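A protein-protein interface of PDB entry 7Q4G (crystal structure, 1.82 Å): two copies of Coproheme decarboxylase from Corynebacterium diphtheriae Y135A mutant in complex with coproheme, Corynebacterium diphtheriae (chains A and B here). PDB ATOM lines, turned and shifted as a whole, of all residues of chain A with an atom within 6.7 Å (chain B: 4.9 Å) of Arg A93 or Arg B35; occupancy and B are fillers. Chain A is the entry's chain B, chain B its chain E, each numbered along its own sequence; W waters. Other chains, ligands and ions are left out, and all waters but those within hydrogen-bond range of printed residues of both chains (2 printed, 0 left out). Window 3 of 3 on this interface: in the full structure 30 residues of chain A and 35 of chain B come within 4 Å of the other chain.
Water W1 lies within hydrogen-bond range of O of Pro B236 and O of Arg A93. Water W2 bridges the backbone carbonyl oxygen of Val B234 (2.8 Å) and the backbone carbonyl oxygen of Ala A89 (2.9 Å).
Printed residues of chain B that touch a printed residue of chain A: Arg B35, Asn B233, Val B234, Leu B235 and Pro B236. Along chain B the printed residues that touch a printed residue of chain A span positions 35 to 236. Printed residues of chain A that touch a printed residue of chain B: Ala A89, Arg A92 and Arg A93. Hydrophobic or aromatic side chains of chain A that line the printed part of chain B: Ala A89. Among the printed residues, 7 pairs touch across the chains.
No position is printed for both chains.
The backbone carbonyl oxygen (O) of Val B234 is in hydrogen-bond range of the guanidinium group (NH1) of Arg A93.
The guanidinium group (NH1) of Arg B35 lies within hydrogen-bond range of the backbone carbonyl oxygen (O) of Val B232 (2.8 Å). The side-chain amide nitrogen (NE2) of Gln A99 lies within hydrogen-bond range of the backbone carbonyl oxygen (O) of Arg A93. The backbone carbonyl oxygen (O) of Leu B235 lies within hydrogen-bond range of the guanidinium group (NH1) of Arg B35. The guanidinium group of Arg A93 lies close to the backbone carbonyl oxygen of Ala A89 (3.4 Å). NE of Arg A93 is in salt-bridge range of OE2 of Glu A94, at 3.3 Å. NE of Arg B35 sits at hydrogen-bond distance from O of Gly B32, at 2.8 Å.
Ala A89 touches Val B234. Arg A92 touches Pro B236. Arg A93 touches Arg B35 (CG to NH2, 3.9 Å). Arg A93 touches Asn B233 (CD to O, 3.6 Å). CD of Arg A93 touches O of Leu B235 (3.3 Å). O of Pro B236 touches CG of Arg A93, 3.5 Å away.
Of the printed residues of chain B, Arg A92 touches Pro B236. Arg A93 touches five residues of chain B. Leu B31 touches none of the printed residues of chain A. Of chain A, only Arg A93 comes within 4 Å of Arg B35. Glu B37 touches none of the printed residues of chain A. Of the printed residues of chain A, Val B234 touches Ala A89 and Arg A93. Printed residues of chain A within 4 Å of Leu B235: Arg A93. The nearest printed residue of chain A that does not touch Arg B35 is Glu A94 (7.4 Å). The nearest printed residue of chain A that does not touch Val B234 is Arg A90 (5.8 Å).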
ATOM      1  N   ALA A  86       7.722   9.826  27.934  1.00  0.00           N
ATOM      2  CA  ALA A  86       6.568  10.222  27.136  1.00  0.00           C
ATOM      3  C   ALA A  86       5.925  11.501  27.656  1.00  0.00           C
ATOM      4  O   ALA A  86       5.618  12.423  26.873  1.00  0.00           O
ATOM      5  CB  ALA A  86       5.518   9.083  27.100  1.00  0.00           C
ATOM      6  N   PHE A  88       7.134  13.871  29.753  1.00  0.00           N
ATOM      7  CA  PHE A  88       8.084  14.982  29.568  1.00  0.00           C
ATOM      8  C   PHE A  88       8.044  15.491  28.131  1.00  0.00           C
ATOM      9  O   PHE A  88       7.815  16.675  27.892  1.00  0.00           O
ATOM     10  CB  PHE A  88       9.462  14.527  29.931  1.00  0.00           C
ATOM     11  CG  PHE A  88      10.550  15.530  29.585  1.00  0.00           C
ATOM     12  CD1 PHE A  88      10.840  16.550  30.432  1.00  0.00           C
ATOM     13  CD2 PHE A  88      11.292  15.386  28.398  1.00  0.00           C
ATOM     14  CE1 PHE A  88      11.863  17.465  30.135  1.00  0.00           C
ATOM     15  CE2 PHE A  88      12.280  16.278  28.082  1.00  0.00           C
ATOM     16  CZ  PHE A  88      12.570  17.336  28.929  1.00  0.00           C
ATOM     17  N   ALA A  89       8.251  14.603  27.171  1.00  0.00           N
ATOM     18  CA  ALA A  89       8.206  14.982  25.765  1.00  0.00           C
ATOM     19  C   ALA A  89       6.854  15.556  25.381  1.00  0.00           C
ATOM     20  O   ALA A  89       6.769  16.484  24.558  1.00  0.00           O
ATOM     21  CB  ALA A  89       8.517  13.749  24.884  1.00  0.00           C
ATOM     22  N   ARG A  90       5.774  15.000  25.942  1.00  0.00           N
ATOM     23  CA  ARG A  90       4.440  15.506  25.624  1.00  0.00           C
ATOM     24  C   ARG A  90       4.269  16.933  26.139  1.00  0.00           C
ATOM     25  O   ARG A  90       3.813  17.819  25.418  1.00  0.00           O
ATOM     26  CB  ARG A  90       3.380  14.572  26.238  1.00  0.00           C
ATOM     27  CG  ARG A  90       1.955  14.934  25.895  1.00  0.00           C
ATOM     28  CD  ARG A  90       0.968  13.879  26.391  1.00  0.00           C
ATOM     29  NE  ARG A  90       1.213  12.547  25.842  1.00  0.00           N
ATOM     30  CZ  ARG A  90       1.813  11.545  26.476  1.00  0.00           C
ATOM     31  NH1 ARG A  90       2.238  11.659  27.744  1.00  0.00           N
ATOM     32  NH2 ARG A  90       1.974  10.386  25.836  1.00  0.00           N
ATOM     33  N   PHE A  91       4.666  17.174  27.380  1.00  0.00           N
ATOM     34  CA  PHE A  91       4.632  18.528  27.922  1.00  0.00           C
ATOM     35  C   PHE A  91       5.315  19.510  26.982  1.00  0.00           C
ATOM     36  O   PHE A  91       4.764  20.557  26.637  1.00  0.00           O
ATOM     37  CB  PHE A  91       5.301  18.541  29.297  1.00  0.00           C
ATOM     38  CG  PHE A  91       5.288  19.881  29.950  1.00  0.00           C
ATOM     39  CD1 PHE A  91       4.081  20.447  30.369  1.00  0.00           C
ATOM     40  CD2 PHE A  91       6.458  20.578  30.150  1.00  0.00           C
ATOM     41  CE1 PHE A  91       4.078  21.702  30.967  1.00  0.00           C
ATOM     42  CE2 PHE A  91       6.446  21.827  30.739  1.00  0.00           C
ATOM     43  CZ  PHE A  91       5.273  22.378  31.152  1.00  0.00           C
ATOM     44  N   ARG A  92       6.527  19.163  26.508  1.00  0.00           N
ATOM     45  CA  ARG A  92       7.276  20.113  25.701  1.00  0.00           C
ATOM     46  C   ARG A  92       6.697  20.291  24.319  1.00  0.00           C
ATOM     47  O   ARG A  92       6.857  21.371  23.715  1.00  0.00           O
ATOM     48  CB  ARG A  92       8.726  19.637  25.545  1.00  0.00           C
ATOM     49  CG  ARG A  92       9.496  19.620  26.807  1.00  0.00           C
ATOM     50  CD  ARG A  92      10.893  19.120  26.537  1.00  0.00           C
ATOM     51  NE  ARG A  92      11.680  20.065  25.764  1.00  0.00           N
ATOM     52  CZ  ARG A  92      12.770  19.733  25.078  1.00  0.00           C
ATOM     53  NH1 ARG A  92      13.136  18.459  24.918  1.00  0.00           N
ATOM     54  NH2 ARG A  92      13.532  20.702  24.567  1.00  0.00           N
ATOM     55  N   ARG A  93       6.057  19.244  23.786  1.00  0.00           N
ATOM     56  CA  ARG A  93       5.662  19.216  22.392  1.00  0.00           C
ATOM     57  C   ARG A  93       4.227  19.690  22.193  1.00  0.00           C
ATOM     58  O   ARG A  93       3.941  20.311  21.175  1.00  0.00           O
ATOM     59  CB  ARG A  93       5.804  17.797  21.832  1.00  0.00           C
ATOM     60  CG  ARG A  93       5.609  17.670  20.349  1.00  0.00           C
ATOM     61  CD  ARG A  93       5.636  16.205  19.886  1.00  0.00           C
ATOM     62  NE  ARG A  93       4.621  15.381  20.556  1.00  0.00           N
ATOM     63  CZ  ARG A  93       4.853  14.558  21.577  1.00  0.00           C
ATOM     64  NH1 ARG A  93       6.063  14.308  22.002  1.00  0.00           N
ATOM     65  NH2 ARG A  93       3.828  13.972  22.189  1.00  0.00           N
ATOM     66  N   GLU A  94       3.337  19.404  23.138  1.00  0.00           N
ATOM     67  CA  GLU A  94       1.901  19.551  22.925  1.00  0.00           C
ATOM     68  C   GLU A  94       1.235  20.512  23.895  1.00  0.00           C
ATOM     69  O   GLU A  94      -0.003  20.475  24.033  1.00  0.00           O
ATOM     70  CB  GLU A  94       1.229  18.171  23.029  1.00  0.00           C
ATOM     71  CG  GLU A  94       2.001  17.030  22.396  1.00  0.00           C
ATOM     72  CD  GLU A  94       1.121  16.026  21.702  1.00  0.00           C
ATOM     73  OE1 GLU A  94       0.166  15.503  22.356  1.00  0.00           O
ATOM     74  OE2 GLU A  94       1.384  15.742  20.514  1.00  0.00           O
ATOM     75  N   THR A  95       2.012  21.344  24.601  1.00  0.00           N
ATOM     76  CA  THR A  95       1.443  22.421  25.421  1.00  0.00           C
ATOM     77  C   THR A  95       2.232  23.709  25.196  1.00  0.00           C
ATOM     78  O   THR A  95       3.475  23.693  25.129  1.00  0.00           O
ATOM     79  CB  THR A  95       1.450  22.112  26.929  1.00  0.00           C
ATOM     80  OG1 THR A  95       2.782  22.234  27.410  1.00  0.00           O
ATOM     81  CG2 THR A  95       0.949  20.702  27.198  1.00  0.00           C
ATOM     82  N   VAL A  96       1.504  24.812  25.060  1.00  0.00           N
ATOM     83  CA  VAL A  96       2.139  26.111  24.876  1.00  0.00           C
ATOM     84  C   VAL A  96       3.119  26.381  26.006  1.00  0.00           C
ATOM     85  O   VAL A  96       4.197  26.926  25.795  1.00  0.00           O
ATOM     86  CB  VAL A  96       1.062  27.212  24.776  1.00  0.00           C
ATOM     87  CG1 VAL A  96       1.686  28.541  24.451  1.00  0.00           C
ATOM     88  CG2 VAL A  96       0.025  26.874  23.722  1.00  0.00           C
ATOM     89  N   GLY A  98       4.890  24.269  27.640  1.00  0.00           N
ATOM     90  CA  GLY A  98       6.112  23.565  27.331  1.00  0.00           C
ATOM     91  C   GLY A  98       6.821  24.132  26.124  1.00  0.00           C
ATOM     92  O   GLY A  98       8.051  24.137  26.072  1.00  0.00           O
ATOM     93  N   GLN A  99       6.066  24.670  25.158  1.00  0.00           N
ATOM     94  CA  GLN A  99       6.683  25.281  23.978  1.00  0.00           C
ATOM     95  C   GLN A  99       7.380  26.603  24.315  1.00  0.00           C
ATOM     96  O   GLN A  99       8.330  26.983  23.650  1.00  0.00           O
ATOM     97  CB  GLN A  99       5.622  25.503  22.912  1.00  0.00           C
ATOM     98  CG  GLN A  99       5.116  24.235  22.266  1.00  0.00           C
ATOM     99  CD  GLN A  99       3.825  24.476  21.507  1.00  0.00           C
ATOM    100  OE1 GLN A  99       3.397  25.626  21.340  1.00  0.00           O
ATOM    101  NE2 GLN A  99       3.185  23.388  21.033  1.00  0.00           N
ATOM    102  N   LEU B  31      11.507  22.156  13.950  1.00  0.00           N
ATOM    103  CA  LEU B  31      10.932  20.996  13.268  1.00  0.00           C
ATOM    104  C   LEU B  31       9.500  21.251  12.831  1.00  0.00           C
ATOM    105  O   LEU B  31       9.072  20.771  11.776  1.00  0.00           O
ATOM    106  CB  LEU B  31      10.990  19.772  14.183  1.00  0.00           C
ATOM    107  CG  LEU B  31      10.960  18.398  13.516  1.00  0.00           C
ATOM    108  CD1 LEU B  31      12.115  18.168  12.579  1.00  0.00           C
ATOM    109  CD2 LEU B  31      10.941  17.339  14.618  1.00  0.00           C
ATOM    110  N   GLY B  32       8.747  21.999  13.614  1.00  0.00           N
ATOM    111  CA  GLY B  32       7.346  22.214  13.291  1.00  0.00           C
ATOM    112  C   GLY B  32       6.526  20.957  13.547  1.00  0.00           C
ATOM    113  O   GLY B  32       6.981  19.977  14.127  1.00  0.00           O
ATOM    114  N   SER B  33       5.287  21.015  13.111  1.00  0.00           N
ATOM    115  CA  SER B  33       4.342  19.934  13.324  1.00  0.00           C
ATOM    116  C   SER B  33       4.046  19.129  12.056  1.00  0.00           C
ATOM    117  O   SER B  33       3.292  18.150  12.124  1.00  0.00           O
ATOM    118  CB  SER B  33       3.037  20.501  13.890  1.00  0.00           C
ATOM    119  OG  SER B  33       2.645  21.648  13.166  1.00  0.00           O
ATOM    120  N   ASP B  34       4.610  19.512  10.911  1.00  0.00           N
ATOM    121  CA  ASP B  34       4.436  18.788   9.656  1.00  0.00           C
ATOM    122  C   ASP B  34       5.745  18.056   9.368  1.00  0.00           C
ATOM    123  O   ASP B  34       6.661  18.603   8.745  1.00  0.00           O
ATOM    124  CB  ASP B  34       4.058  19.730   8.532  1.00  0.00           C
ATOM    125  CG  ASP B  34       3.262  19.034   7.442  1.00  0.00           C
ATOM    126  OD1 ASP B  34       2.646  19.740   6.611  1.00  0.00           O
ATOM    127  OD2 ASP B  34       3.267  17.781   7.415  1.00  0.00           O
ATOM    128  N   ARG B  35       5.828  16.811   9.832  1.00  0.00           N
ATOM    129  CA  ARG B  35       7.079  16.056   9.849  1.00  0.00           C
ATOM    130  C   ARG B  35       7.079  14.845   8.918  1.00  0.00           C
ATOM    131  O   ARG B  35       8.055  14.100   8.902  1.00  0.00           O
ATOM    132  CB  ARG B  35       7.374  15.596  11.281  1.00  0.00           C
ATOM    133  CG  ARG B  35       7.192  16.687  12.319  1.00  0.00           C
ATOM    134  CD  ARG B  35       7.496  16.210  13.717  1.00  0.00           C
ATOM    135  NE  ARG B  35       7.328  17.285  14.707  1.00  0.00           N
ATOM    136  CZ  ARG B  35       7.553  17.152  16.008  1.00  0.00           C
ATOM    137  NH1 ARG B  35       8.018  16.018  16.519  1.00  0.00           N
ATOM    138  NH2 ARG B  35       7.286  18.178  16.824  1.00  0.00           N
ATOM    139  N   ALA B  36       6.001  14.631   8.149  1.00  0.00           N
ATOM    140  CA  ALA B  36       5.927  13.448   7.306  1.00  0.00           C
ATOM    141  C   ALA B  36       7.078  13.419   6.297  1.00  0.00           C
ATOM    142  O   ALA B  36       7.828  12.447   6.220  1.00  0.00           O
ATOM    143  CB  ALA B  36       4.576  13.412   6.593  1.00  0.00           C
ATOM    144  N   GLU B  37       7.227  14.488   5.512  1.00  0.00           N
ATOM    145  CA  GLU B  37       8.328  14.567   4.557  1.00  0.00           C
ATOM    146  C   GLU B  37       9.680  14.471   5.255  1.00  0.00           C
ATOM    147  O   GLU B  37      10.624  13.833   4.742  1.00  0.00           O
ATOM    148  CB  GLU B  37       8.230  15.868   3.761  1.00  0.00           C
ATOM    149  CG  GLU B  37       7.376  15.771   2.498  1.00  0.00           C
ATOM    150  CD  GLU B  37       7.451  17.030   1.637  1.00  0.00           C
ATOM    151  OE1 GLU B  37       6.417  17.422   1.054  1.00  0.00           O
ATOM    152  OE2 GLU B  37       8.546  17.627   1.555  1.00  0.00           O
ATOM    153  N   ILE B  38       9.806  15.085   6.439  1.00  0.00           N
ATOM    154  CA  ILE B  38      11.080  15.015   7.165  1.00  0.00           C
ATOM    155  C   ILE B  38      11.405  13.579   7.547  1.00  0.00           C
ATOM    156  O   ILE B  38      12.553  13.133   7.428  1.00  0.00           O
ATOM    157  CB  ILE B  38      11.028  15.935   8.410  1.00  0.00           C
ATOM    158  CG1 ILE B  38      11.154  17.392   7.978  1.00  0.00           C
ATOM    159  CG2 ILE B  38      12.079  15.561   9.415  1.00  0.00           C
ATOM    160  CD1 ILE B  38      10.479  18.387   8.933  1.00  0.00           C
ATOM    161  N   VAL B  39      10.404  12.829   8.023  1.00  0.00           N
ATOM    162  CA  VAL B  39      10.634  11.421   8.369  1.00  0.00           C
ATOM    163  C   VAL B  39      11.070  10.621   7.129  1.00  0.00           C
ATOM    164  O   VAL B  39      12.092   9.937   7.137  1.00  0.00           O
ATOM    165  CB  VAL B  39       9.359  10.819   8.998  1.00  0.00           C
ATOM    166  CG1 VAL B  39       9.467   9.312   9.106  1.00  0.00           C
ATOM    167  CG2 VAL B  39       9.099  11.463  10.351  1.00  0.00           C
ATOM    168  N   VAL B 232      11.430  10.858  15.471  1.00  0.00           N
ATOM    169  CA  VAL B 232      11.072  12.191  15.015  1.00  0.00           C
ATOM    170  C   VAL B 232       9.756  12.642  15.631  1.00  0.00           C
ATOM    171  O   VAL B 232       9.601  13.819  15.998  1.00  0.00           O
ATOM    172  CB  VAL B 232      11.025  12.235  13.482  1.00  0.00           C
ATOM    173  CG1 VAL B 232      10.431  13.545  13.009  1.00  0.00           C
ATOM    174  CG2 VAL B 232      12.406  11.998  12.901  1.00  0.00           C
ATOM    175  N   ASN B 233       8.787  11.720  15.771  1.00  0.00           N
ATOM    176  CA  ASN B 233       7.463  12.120  16.262  1.00  0.00           C
ATOM    177  C   ASN B 233       7.464  12.532  17.746  1.00  0.00           C
ATOM    178  O   ASN B 233       6.533  13.210  18.177  1.00  0.00           O
ATOM    179  CB  ASN B 233       6.422  10.984  16.052  1.00  0.00           C
ATOM    180  CG  ASN B 233       6.158  10.721  14.605  1.00  0.00           C
ATOM    181  OD1 ASN B 233       6.124  11.652  13.789  1.00  0.00           O
ATOM    182  ND2 ASN B 233       5.902   9.450  14.260  1.00  0.00           N
ATOM    183  N   VAL B 234       8.472  12.179  18.522  1.00  0.00           N
ATOM    184  CA  VAL B 234       8.502  12.608  19.908  1.00  0.00           C
ATOM    185  C   VAL B 234       9.188  13.960  20.120  1.00  0.00           C
ATOM    186  O   VAL B 234       8.961  14.597  21.169  1.00  0.00           O
ATOM    187  CB  VAL B 234       9.180  11.569  20.824  1.00  0.00           C
ATOM    188  CG1 VAL B 234       8.352  10.310  20.875  1.00  0.00           C
ATOM    189  CG2 VAL B 234      10.557  11.262  20.387  1.00  0.00           C
ATOM    190  N   LEU B 235       9.935  14.453  19.137  1.00  0.00           N
ATOM    191  CA  LEU B 235      10.803  15.613  19.376  1.00  0.00           C
ATOM    192  C   LEU B 235       9.969  16.857  19.644  1.00  0.00           C
ATOM    193  O   LEU B 235       8.815  16.967  19.197  1.00  0.00           O
ATOM    194  CB  LEU B 235      11.727  15.852  18.167  1.00  0.00           C
ATOM    195  CG  LEU B 235      12.708  14.731  17.863  1.00  0.00           C
ATOM    196  CD1 LEU B 235      13.457  14.982  16.575  1.00  0.00           C
ATOM    197  CD2 LEU B 235      13.742  14.599  18.994  1.00  0.00           C
ATOM    198  N   PRO B 236      10.524  17.822  20.376  1.00  0.00           N
ATOM    199  CA  PRO B 236       9.708  18.961  20.821  1.00  0.00           C
ATOM    200  C   PRO B 236       9.093  19.750  19.706  1.00  0.00           C
ATOM    201  O   PRO B 236       7.963  20.262  19.862  1.00  0.00           O
ATOM    202  CB  PRO B 236      10.705  19.807  21.637  1.00  0.00           C
ATOM    203  CG  PRO B 236      12.023  19.324  21.251  1.00  0.00           C
ATOM    204  CD  PRO B 236      11.866  17.879  20.947  1.00  0.00           C
ATOM    205  N   GLY B 237       9.766  19.881  18.580  1.00  0.00           N
ATOM    206  CA  GLY B 237       9.126  20.637  17.488  1.00  0.00           C
ATOM    207  C   GLY B 237       9.438  22.120  17.518  1.00  0.00           C
ATOM    208  O   GLY B 237       9.209  22.867  16.541  1.00  0.00           O
ATOM    209  OXT GLY B 237       9.952  22.619  18.522  1.00  0.00           O
HETATM  210  O   HOH W   1       5.980  21.551  19.345  1.00  0.00           O
HETATM  211  O   HOH W   2       9.240  16.758  22.993  1.00  0.00           O
